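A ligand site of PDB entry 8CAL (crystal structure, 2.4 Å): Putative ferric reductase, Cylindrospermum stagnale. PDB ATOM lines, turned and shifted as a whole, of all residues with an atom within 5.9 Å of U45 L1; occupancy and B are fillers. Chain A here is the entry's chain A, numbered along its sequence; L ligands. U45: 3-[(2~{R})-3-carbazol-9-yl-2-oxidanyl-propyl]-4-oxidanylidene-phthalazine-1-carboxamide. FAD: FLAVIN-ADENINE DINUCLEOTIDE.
OE2 of Glu 281 sits at hydrogen-bond distance from NAA of U45 L1.
SG of Cys 258 lies close to OAI of U45 L1, at 3.7 Å.
The backbone NH of Thr 52 is in hydrogen-bond range of a nitrogen (N5) of FAD L2 (3.1 Å).
The side-chain hydroxyl (OG1) of Thr 52 sits at hydrogen-bond distance from a nitrogen (N5) of FAD L2, at 3.3 Å.
OG1 of Thr 131 sits at hydrogen-bond distance from O4 of FAD L2, 3.0 Å away.
O of Pro 50 lies within hydrogen-bond range of O2' of FAD L2, at 2.5 Å.
The side-chain hydroxyl (OG1) of Thr 52 lies close to the side-chain hydroxyl (OG1) of Thr 131 (3.5 Å).
SG of Cys 258 lies within hydrogen-bond range of O of Gly 129, 3.3 Å away.
The backbone carbonyl oxygen of Ile 128 lies close to the side-chain hydroxyl of Thr 131 (3.1 Å).
Tyr 35 touches U45 L1 (CE1 to OAC, 3.2 Å).
Thr 52 touches U45 L1.
Thr 110 touches U45 L1.
Ile 128 touches U45 L1 (O to CAQ, 3.6 Å).
Gly 129 touches U45 L1.
Thr 131 touches U45 L1.
Hydrophobic or aromatic side chains within 4 Å of U45 L1: Tyr 35.
Eight residues have an atom within 4 Å of U45 L1: Tyr 35, Thr 52, Thr 110, Ile 128, Gly 129, Thr 131, Cys 258 and Glu 281.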
ATOM      1  N   TYR A  35      14.563  27.605 -13.319  1.00  0.00           N
ATOM      2  CA  TYR A  35      14.691  26.476 -12.379  1.00  0.00           C
ATOM      3  C   TYR A  35      14.579  27.034 -10.955  1.00  0.00           C
ATOM      4  O   TYR A  35      14.480  28.291 -10.734  1.00  0.00           O
ATOM      5  CB  TYR A  35      15.957  25.690 -12.692  1.00  0.00           C
ATOM      6  CG  TYR A  35      17.254  26.414 -12.475  1.00  0.00           C
ATOM      7  CD1 TYR A  35      17.781  27.270 -13.423  1.00  0.00           C
ATOM      8  CD2 TYR A  35      17.996  26.199 -11.319  1.00  0.00           C
ATOM      9  CE1 TYR A  35      18.987  27.925 -13.204  1.00  0.00           C
ATOM     10  CE2 TYR A  35      19.213  26.824 -11.103  1.00  0.00           C
ATOM     11  CZ  TYR A  35      19.710  27.683 -12.052  1.00  0.00           C
ATOM     12  OH  TYR A  35      20.909  28.274 -11.851  1.00  0.00           O
ATOM     13  N   PHE A  37      15.915  25.786  -6.663  1.00  0.00           N
ATOM     14  CA  PHE A  37      16.554  24.791  -5.752  1.00  0.00           C
ATOM     15  C   PHE A  37      15.505  24.345  -4.749  1.00  0.00           C
ATOM     16  O   PHE A  37      14.665  25.141  -4.318  1.00  0.00           O
ATOM     17  CB  PHE A  37      17.807  25.347  -5.072  1.00  0.00           C
ATOM     18  CG  PHE A  37      19.022  25.432  -5.956  1.00  0.00           C
ATOM     19  CD1 PHE A  37      19.209  26.533  -6.761  1.00  0.00           C
ATOM     20  CD2 PHE A  37      19.979  24.436  -5.927  1.00  0.00           C
ATOM     21  CE1 PHE A  37      20.315  26.612  -7.586  1.00  0.00           C
ATOM     22  CE2 PHE A  37      21.095  24.507  -6.744  1.00  0.00           C
ATOM     23  CZ  PHE A  37      21.237  25.575  -7.597  1.00  0.00           C
ATOM     24  N   PRO A  50      18.768  21.457  -7.652  1.00  0.00           N
ATOM     25  CA  PRO A  50      18.084  22.274  -8.650  1.00  0.00           C
ATOM     26  C   PRO A  50      17.212  21.432  -9.603  1.00  0.00           C
ATOM     27  O   PRO A  50      17.610  20.355 -10.078  1.00  0.00           O
ATOM     28  CB  PRO A  50      19.262  22.891  -9.383  1.00  0.00           C
ATOM     29  CG  PRO A  50      20.314  21.784  -9.384  1.00  0.00           C
ATOM     30  CD  PRO A  50      20.160  21.109  -8.028  1.00  0.00           C
ATOM     31  N   THR A  52      14.373  22.180 -12.968  1.00  0.00           N
ATOM     32  CA  THR A  52      13.604  23.032 -13.895  1.00  0.00           C
ATOM     33  C   THR A  52      12.149  22.999 -13.447  1.00  0.00           C
ATOM     34  O   THR A  52      11.633  21.892 -13.122  1.00  0.00           O
ATOM     35  CB  THR A  52      13.685  22.491 -15.329  1.00  0.00           C
ATOM     36  OG1 THR A  52      15.047  22.387 -15.752  1.00  0.00           O
ATOM     37  CG2 THR A  52      12.882  23.368 -16.255  1.00  0.00           C
ATOM     38  N   GLY A 109      17.216  32.002 -13.649  1.00  0.00           N
ATOM     39  CA  GLY A 109      17.021  32.147 -15.097  1.00  0.00           C
ATOM     40  C   GLY A 109      17.982  31.282 -15.875  1.00  0.00           C
ATOM     41  O   GLY A 109      18.926  30.817 -15.333  1.00  0.00           O
ATOM     42  N   THR A 110      17.668  31.044 -17.148  1.00  0.00           N
ATOM     43  CA  THR A 110      18.515  30.331 -18.122  1.00  0.00           C
ATOM     44  C   THR A 110      18.371  31.121 -19.400  1.00  0.00           C
ATOM     45  O   THR A 110      17.365  31.830 -19.555  1.00  0.00           O
ATOM     46  CB  THR A 110      18.137  28.857 -18.334  1.00  0.00           C
ATOM     47  OG1 THR A 110      16.862  28.742 -18.962  1.00  0.00           O
ATOM     48  CG2 THR A 110      18.118  28.079 -17.033  1.00  0.00           C
ATOM     49  N   PRO A 111      19.386  31.093 -20.276  1.00  0.00           N
ATOM     50  CA  PRO A 111      19.285  31.779 -21.566  1.00  0.00           C
ATOM     51  C   PRO A 111      18.166  31.224 -22.472  1.00  0.00           C
ATOM     52  O   PRO A 111      17.706  31.970 -23.270  1.00  0.00           O
ATOM     53  CB  PRO A 111      20.699  31.640 -22.112  1.00  0.00           C
ATOM     54  CG  PRO A 111      21.234  30.391 -21.478  1.00  0.00           C
ATOM     55  CD  PRO A 111      20.688  30.454 -20.076  1.00  0.00           C
ATOM     56  N   ILE A 128      15.473  13.730 -19.599  1.00  0.00           N
ATOM     57  CA  ILE A 128      14.692  14.638 -18.704  1.00  0.00           C
ATOM     58  C   ILE A 128      15.082  16.103 -19.004  1.00  0.00           C
ATOM     59  O   ILE A 128      14.378  17.042 -18.537  1.00  0.00           O
ATOM     60  CB  ILE A 128      14.902  14.230 -17.224  1.00  0.00           C
ATOM     61  CG1 ILE A 128      13.812  14.794 -16.332  1.00  0.00           C
ATOM     62  CG2 ILE A 128      16.281  14.632 -16.733  1.00  0.00           C
ATOM     63  CD1 ILE A 128      12.489  14.172 -16.575  1.00  0.00           C
ATOM     64  N   GLY A 129      16.144  16.267 -19.795  1.00  0.00           N
ATOM     65  CA  GLY A 129      16.552  17.538 -20.456  1.00  0.00           C
ATOM     66  C   GLY A 129      15.432  18.269 -21.175  1.00  0.00           C
ATOM     67  O   GLY A 129      15.572  19.450 -21.437  1.00  0.00           O
ATOM     68  N   VAL A 130      14.347  17.579 -21.509  1.00  0.00           N
ATOM     69  CA  VAL A 130      13.138  18.192 -22.110  1.00  0.00           C
ATOM     70  C   VAL A 130      12.445  19.198 -21.194  1.00  0.00           C
ATOM     71  O   VAL A 130      11.663  20.004 -21.703  1.00  0.00           O
ATOM     72  CB  VAL A 130      12.175  17.072 -22.498  1.00  0.00           C
ATOM     73  CG1 VAL A 130      11.645  16.376 -21.267  1.00  0.00           C
ATOM     74  CG2 VAL A 130      11.048  17.596 -23.380  1.00  0.00           C
ATOM     75  N   THR A 131      12.641  19.152 -19.896  1.00  0.00           N
ATOM     76  CA  THR A 131      11.736  19.855 -18.955  1.00  0.00           C
ATOM     77  C   THR A 131      11.691  21.356 -19.222  1.00  0.00           C
ATOM     78  O   THR A 131      10.625  21.958 -19.111  1.00  0.00           O
ATOM     79  CB  THR A 131      12.085  19.486 -17.523  1.00  0.00           C
ATOM     80  OG1 THR A 131      13.481  19.699 -17.309  1.00  0.00           O
ATOM     81  CG2 THR A 131      11.783  18.023 -17.275  1.00  0.00           C
ATOM     82  N   PRO A 132      12.796  22.073 -19.478  1.00  0.00           N
ATOM     83  CA  PRO A 132      12.666  23.516 -19.662  1.00  0.00           C
ATOM     84  C   PRO A 132      11.886  23.763 -20.965  1.00  0.00           C
ATOM     85  O   PRO A 132      11.129  24.705 -21.051  1.00  0.00           O
ATOM     86  CB  PRO A 132      14.115  24.005 -19.640  1.00  0.00           C
ATOM     87  CG  PRO A 132      14.935  22.813 -20.068  1.00  0.00           C
ATOM     88  CD  PRO A 132      14.183  21.623 -19.543  1.00  0.00           C
ATOM     89  N   PHE A 257      19.992  24.125 -26.143  1.00  0.00           N
ATOM     90  CA  PHE A 257      20.417  22.745 -25.892  1.00  0.00           C
ATOM     91  C   PHE A 257      20.250  22.450 -24.412  1.00  0.00           C
ATOM     92  O   PHE A 257      20.732  23.174 -23.650  1.00  0.00           O
ATOM     93  CB  PHE A 257      21.887  22.526 -26.244  1.00  0.00           C
ATOM     94  CG  PHE A 257      22.331  21.109 -25.988  1.00  0.00           C
ATOM     95  CD1 PHE A 257      21.698  20.038 -26.617  1.00  0.00           C
ATOM     96  CD2 PHE A 257      23.376  20.844 -25.115  1.00  0.00           C
ATOM     97  CE1 PHE A 257      22.131  18.735 -26.391  1.00  0.00           C
ATOM     98  CE2 PHE A 257      23.799  19.534 -24.896  1.00  0.00           C
ATOM     99  CZ  PHE A 257      23.163  18.471 -25.514  1.00  0.00           C
ATOM    100  N   CYS A 258      19.628  21.349 -24.071  1.00  0.00           N
ATOM    101  CA  CYS A 258      19.663  20.803 -22.719  1.00  0.00           C
ATOM    102  C   CYS A 258      19.938  19.300 -22.794  1.00  0.00           C
ATOM    103  O   CYS A 258      19.010  18.516 -23.095  1.00  0.00           O
ATOM    104  CB  CYS A 258      18.383  21.151 -21.990  1.00  0.00           C
ATOM    105  SG  CYS A 258      18.461  20.578 -20.282  1.00  0.00           S
ATOM    106  N   GLY A 259      21.196  18.910 -22.552  1.00  0.00           N
ATOM    107  CA  GLY A 259      21.597  17.495 -22.599  1.00  0.00           C
ATOM    108  C   GLY A 259      23.078  17.292 -22.395  1.00  0.00           C
ATOM    109  O   GLY A 259      23.796  18.173 -21.929  1.00  0.00           O
ATOM    110  N   GLU A 281      26.693  26.162 -22.148  1.00  0.00           N
ATOM    111  CA  GLU A 281      25.996  25.719 -20.906  1.00  0.00           C
ATOM    112  C   GLU A 281      26.473  24.315 -20.493  1.00  0.00           C
ATOM    113  O   GLU A 281      25.860  23.736 -19.594  1.00  0.00           O
ATOM    114  CB  GLU A 281      24.491  25.695 -21.140  1.00  0.00           C
ATOM    115  CG  GLU A 281      23.864  27.075 -21.280  1.00  0.00           C
ATOM    116  CD  GLU A 281      22.391  27.051 -21.683  1.00  0.00           C
ATOM    117  OE1 GLU A 281      22.093  26.530 -22.776  1.00  0.00           O
ATOM    118  OE2 GLU A 281      21.533  27.464 -20.868  1.00  0.00           O
ATOM    119  N   ASN A 282      27.537  23.791 -21.101  1.00  0.00           N
ATOM    120  CA  ASN A 282      28.052  22.415 -20.850  1.00  0.00           C
ATOM    121  C   ASN A 282      29.566  22.533 -20.716  1.00  0.00           C
ATOM    122  O   ASN A 282      30.188  23.132 -21.617  1.00  0.00           O
ATOM    123  CB  ASN A 282      27.737  21.423 -21.991  1.00  0.00           C
ATOM    124  CG  ASN A 282      26.317  20.899 -21.938  1.00  0.00           C
ATOM    125  OD1 ASN A 282      26.060  19.737 -21.583  1.00  0.00           O
ATOM    126  ND2 ASN A 282      25.395  21.772 -22.304  1.00  0.00           N
HETATM  127  CAM U45 L   1      21.057  17.158 -15.502  1.00  0.00           C
HETATM  128  CAL U45 L   1      22.408  16.981 -15.116  1.00  0.00           C
HETATM  129  CAT U45 L   1      23.252  18.125 -15.153  1.00  0.00           C
HETATM  130  CAJ U45 L   1      22.738  19.407 -15.541  1.00  0.00           C
HETATM  131  CAS U45 L   1      21.426  19.512 -15.876  1.00  0.00           C
HETATM  132  CAN U45 L   1      20.617  18.412 -15.862  1.00  0.00           C
HETATM  133  CAO U45 L   1      19.389  18.819 -16.242  1.00  0.00           C
HETATM  134  CAP U45 L   1      18.249  18.104 -16.376  1.00  0.00           C
HETATM  135  CAQ U45 L   1      17.067  18.737 -16.818  1.00  0.00           C
HETATM  136  CAU U45 L   1      17.126  20.121 -17.066  1.00  0.00           C
HETATM  137  CAV U45 L   1      18.355  20.820 -16.909  1.00  0.00           C
HETATM  138  CBC U45 L   1      19.450  20.158 -16.511  1.00  0.00           C
HETATM  139  NAR U45 L   1      20.694  20.582 -16.269  1.00  0.00           N
HETATM  140  CAK U45 L   1      21.301  21.923 -16.440  1.00  0.00           C
HETATM  141  CAH U45 L   1      22.331  21.779 -17.690  1.00  0.00           C
HETATM  142  OAI U45 L   1      21.434  22.116 -18.774  1.00  0.00           O
HETATM  143  CAD U45 L   1      23.699  22.602 -17.837  1.00  0.00           C
HETATM  144  NAG U45 L   1      23.593  23.541 -16.719  1.00  0.00           N
HETATM  145  NAF U45 L   1      22.779  24.448 -16.891  1.00  0.00           N
HETATM  146  CBD U45 L   1      24.297  23.287 -15.570  1.00  0.00           C
HETATM  147  OBE U45 L   1      25.124  22.347 -15.434  1.00  0.00           O
HETATM  148  CAW U45 L   1      24.065  24.116 -14.492  1.00  0.00           C
HETATM  149  CAX U45 L   1      24.763  23.844 -13.288  1.00  0.00           C
HETATM  150  CAY U45 L   1      24.559  24.650 -12.187  1.00  0.00           C
HETATM  151  CAZ U45 L   1      23.640  25.699 -12.325  1.00  0.00           C
HETATM  152  CBA U45 L   1      22.982  25.965 -13.543  1.00  0.00           C
HETATM  153  CBB U45 L   1      23.175  25.153 -14.651  1.00  0.00           C
HETATM  154  CAE U45 L   1      22.522  25.312 -15.878  1.00  0.00           C
HETATM  155  CAB U45 L   1      21.675  26.340 -16.242  1.00  0.00           C
HETATM  156  OAC U45 L   1      21.058  26.963 -15.398  1.00  0.00           O
HETATM  157  NAA U45 L   1      21.778  26.779 -17.566  1.00  0.00           N
HETATM  158  PA  FAD L   2      23.775  11.678  -7.298  1.00  0.00           P
HETATM  159  O1A FAD L   2      24.472  12.986  -7.256  1.00  0.00           O
HETATM  160  O2A FAD L   2      23.866  10.632  -6.230  1.00  0.00           O
HETATM  161  O5B FAD L   2      24.208  10.995  -8.681  1.00  0.00           O
HETATM  162  C5B FAD L   2      24.190  11.744  -9.926  1.00  0.00           C
HETATM  163  C4B FAD L   2      24.888  10.942 -10.996  1.00  0.00           C
HETATM  164  O4B FAD L   2      26.326  10.939 -10.749  1.00  0.00           O
HETATM  165  C3B FAD L   2      24.508   9.462 -11.080  1.00  0.00           C
HETATM  166  O3B FAD L   2      24.591   9.018 -12.432  1.00  0.00           O
HETATM  167  C2B FAD L   2      25.551   8.815 -10.156  1.00  0.00           C
HETATM  168  O2B FAD L   2      25.839   7.470 -10.430  1.00  0.00           O
HETATM  169  C1B FAD L   2      26.773   9.636 -10.486  1.00  0.00           C
HETATM  170  N9A FAD L   2      27.736   9.655  -9.410  1.00  0.00           N
HETATM  171  C8A FAD L   2      27.506   9.865  -8.067  1.00  0.00           C
HETATM  172  N7A FAD L   2      28.611   9.784  -7.355  1.00  0.00           N
HETATM  173  C5A FAD L   2      29.594   9.492  -8.290  1.00  0.00           C
HETATM  174  C6A FAD L   2      30.985   9.280  -8.170  1.00  0.00           C
HETATM  175  N6A FAD L   2      31.616   9.313  -7.013  1.00  0.00           N
HETATM  176  N1A FAD L   2      31.682   9.016  -9.314  1.00  0.00           N
HETATM  177  C2A FAD L   2      31.023   8.979 -10.483  1.00  0.00           C
HETATM  178  N3A FAD L   2      29.721   9.154 -10.706  1.00  0.00           N
HETATM  179  C4A FAD L   2      29.067   9.413  -9.566  1.00  0.00           C
HETATM  180  N1  FAD L   2      16.985  16.644 -12.985  1.00  0.00           N
HETATM  181  C2  FAD L   2      15.739  16.226 -13.257  1.00  0.00           C
HETATM  182  O2  FAD L   2      15.461  15.071 -13.055  1.00  0.00           O
HETATM  183  N3  FAD L   2      14.757  17.055 -13.740  1.00  0.00           N
HETATM  184  C4  FAD L   2      14.997  18.374 -14.007  1.00  0.00           C
HETATM  185  O4  FAD L   2      14.107  19.074 -14.455  1.00  0.00           O
HETATM  186  C4X FAD L   2      16.284  18.863 -13.686  1.00  0.00           C
HETATM  187  N5  FAD L   2      16.515  20.114 -13.906  1.00  0.00           N
HETATM  188  C5X FAD L   2      17.766  20.549 -13.583  1.00  0.00           C
HETATM  189  C6  FAD L   2      18.014  21.922 -13.779  1.00  0.00           C
HETATM  190  C7  FAD L   2      19.217  22.495 -13.495  1.00  0.00           C
HETATM  191  C7M FAD L   2      19.408  23.978 -13.747  1.00  0.00           C
HETATM  192  C8  FAD L   2      20.239  21.699 -12.973  1.00  0.00           C
HETATM  193  C8M FAD L   2      21.584  22.315 -12.685  1.00  0.00           C
HETATM  194  C9  FAD L   2      20.031  20.322 -12.790  1.00  0.00           C
HETATM  195  C9A FAD L   2      18.794  19.709 -13.073  1.00  0.00           C
HETATM  196  N10 FAD L   2      18.509  18.343 -12.853  1.00  0.00           N
HETATM  197  C10 FAD L   2      17.251  17.909 -13.153  1.00  0.00           C
HETATM  198  C1' FAD L   2      19.462  17.370 -12.178  1.00  0.00           C
HETATM  199  C2' FAD L   2      19.334  17.406 -10.580  1.00  0.00           C
HETATM  200  O2' FAD L   2      19.491  18.786 -10.185  1.00  0.00           O
HETATM  201  C3' FAD L   2      19.982  16.552  -9.433  1.00  0.00           C
HETATM  202  O3' FAD L   2      21.071  16.879  -8.459  1.00  0.00           O
HETATM  203  C4' FAD L   2      20.615  15.299  -9.921  1.00  0.00           C
HETATM  204  O4' FAD L   2      19.933  15.224 -11.166  1.00  0.00           O
HETATM  205  C5' FAD L   2      20.412  14.228  -8.869  1.00  0.00           C
HETATM  206  O5' FAD L   2      21.100  14.305  -7.562  1.00  0.00           O
HETATM  207  P   FAD L   2      21.189  12.906  -6.677  1.00  0.00           P
HETATM  208  O1P FAD L   2      21.718  13.096  -5.329  1.00  0.00           O
HETATM  209  O2P FAD L   2      19.880  12.184  -6.774  1.00  0.00           O
HETATM  210  O3P FAD L   2      22.221  12.011  -7.479  1.00  0.00           O
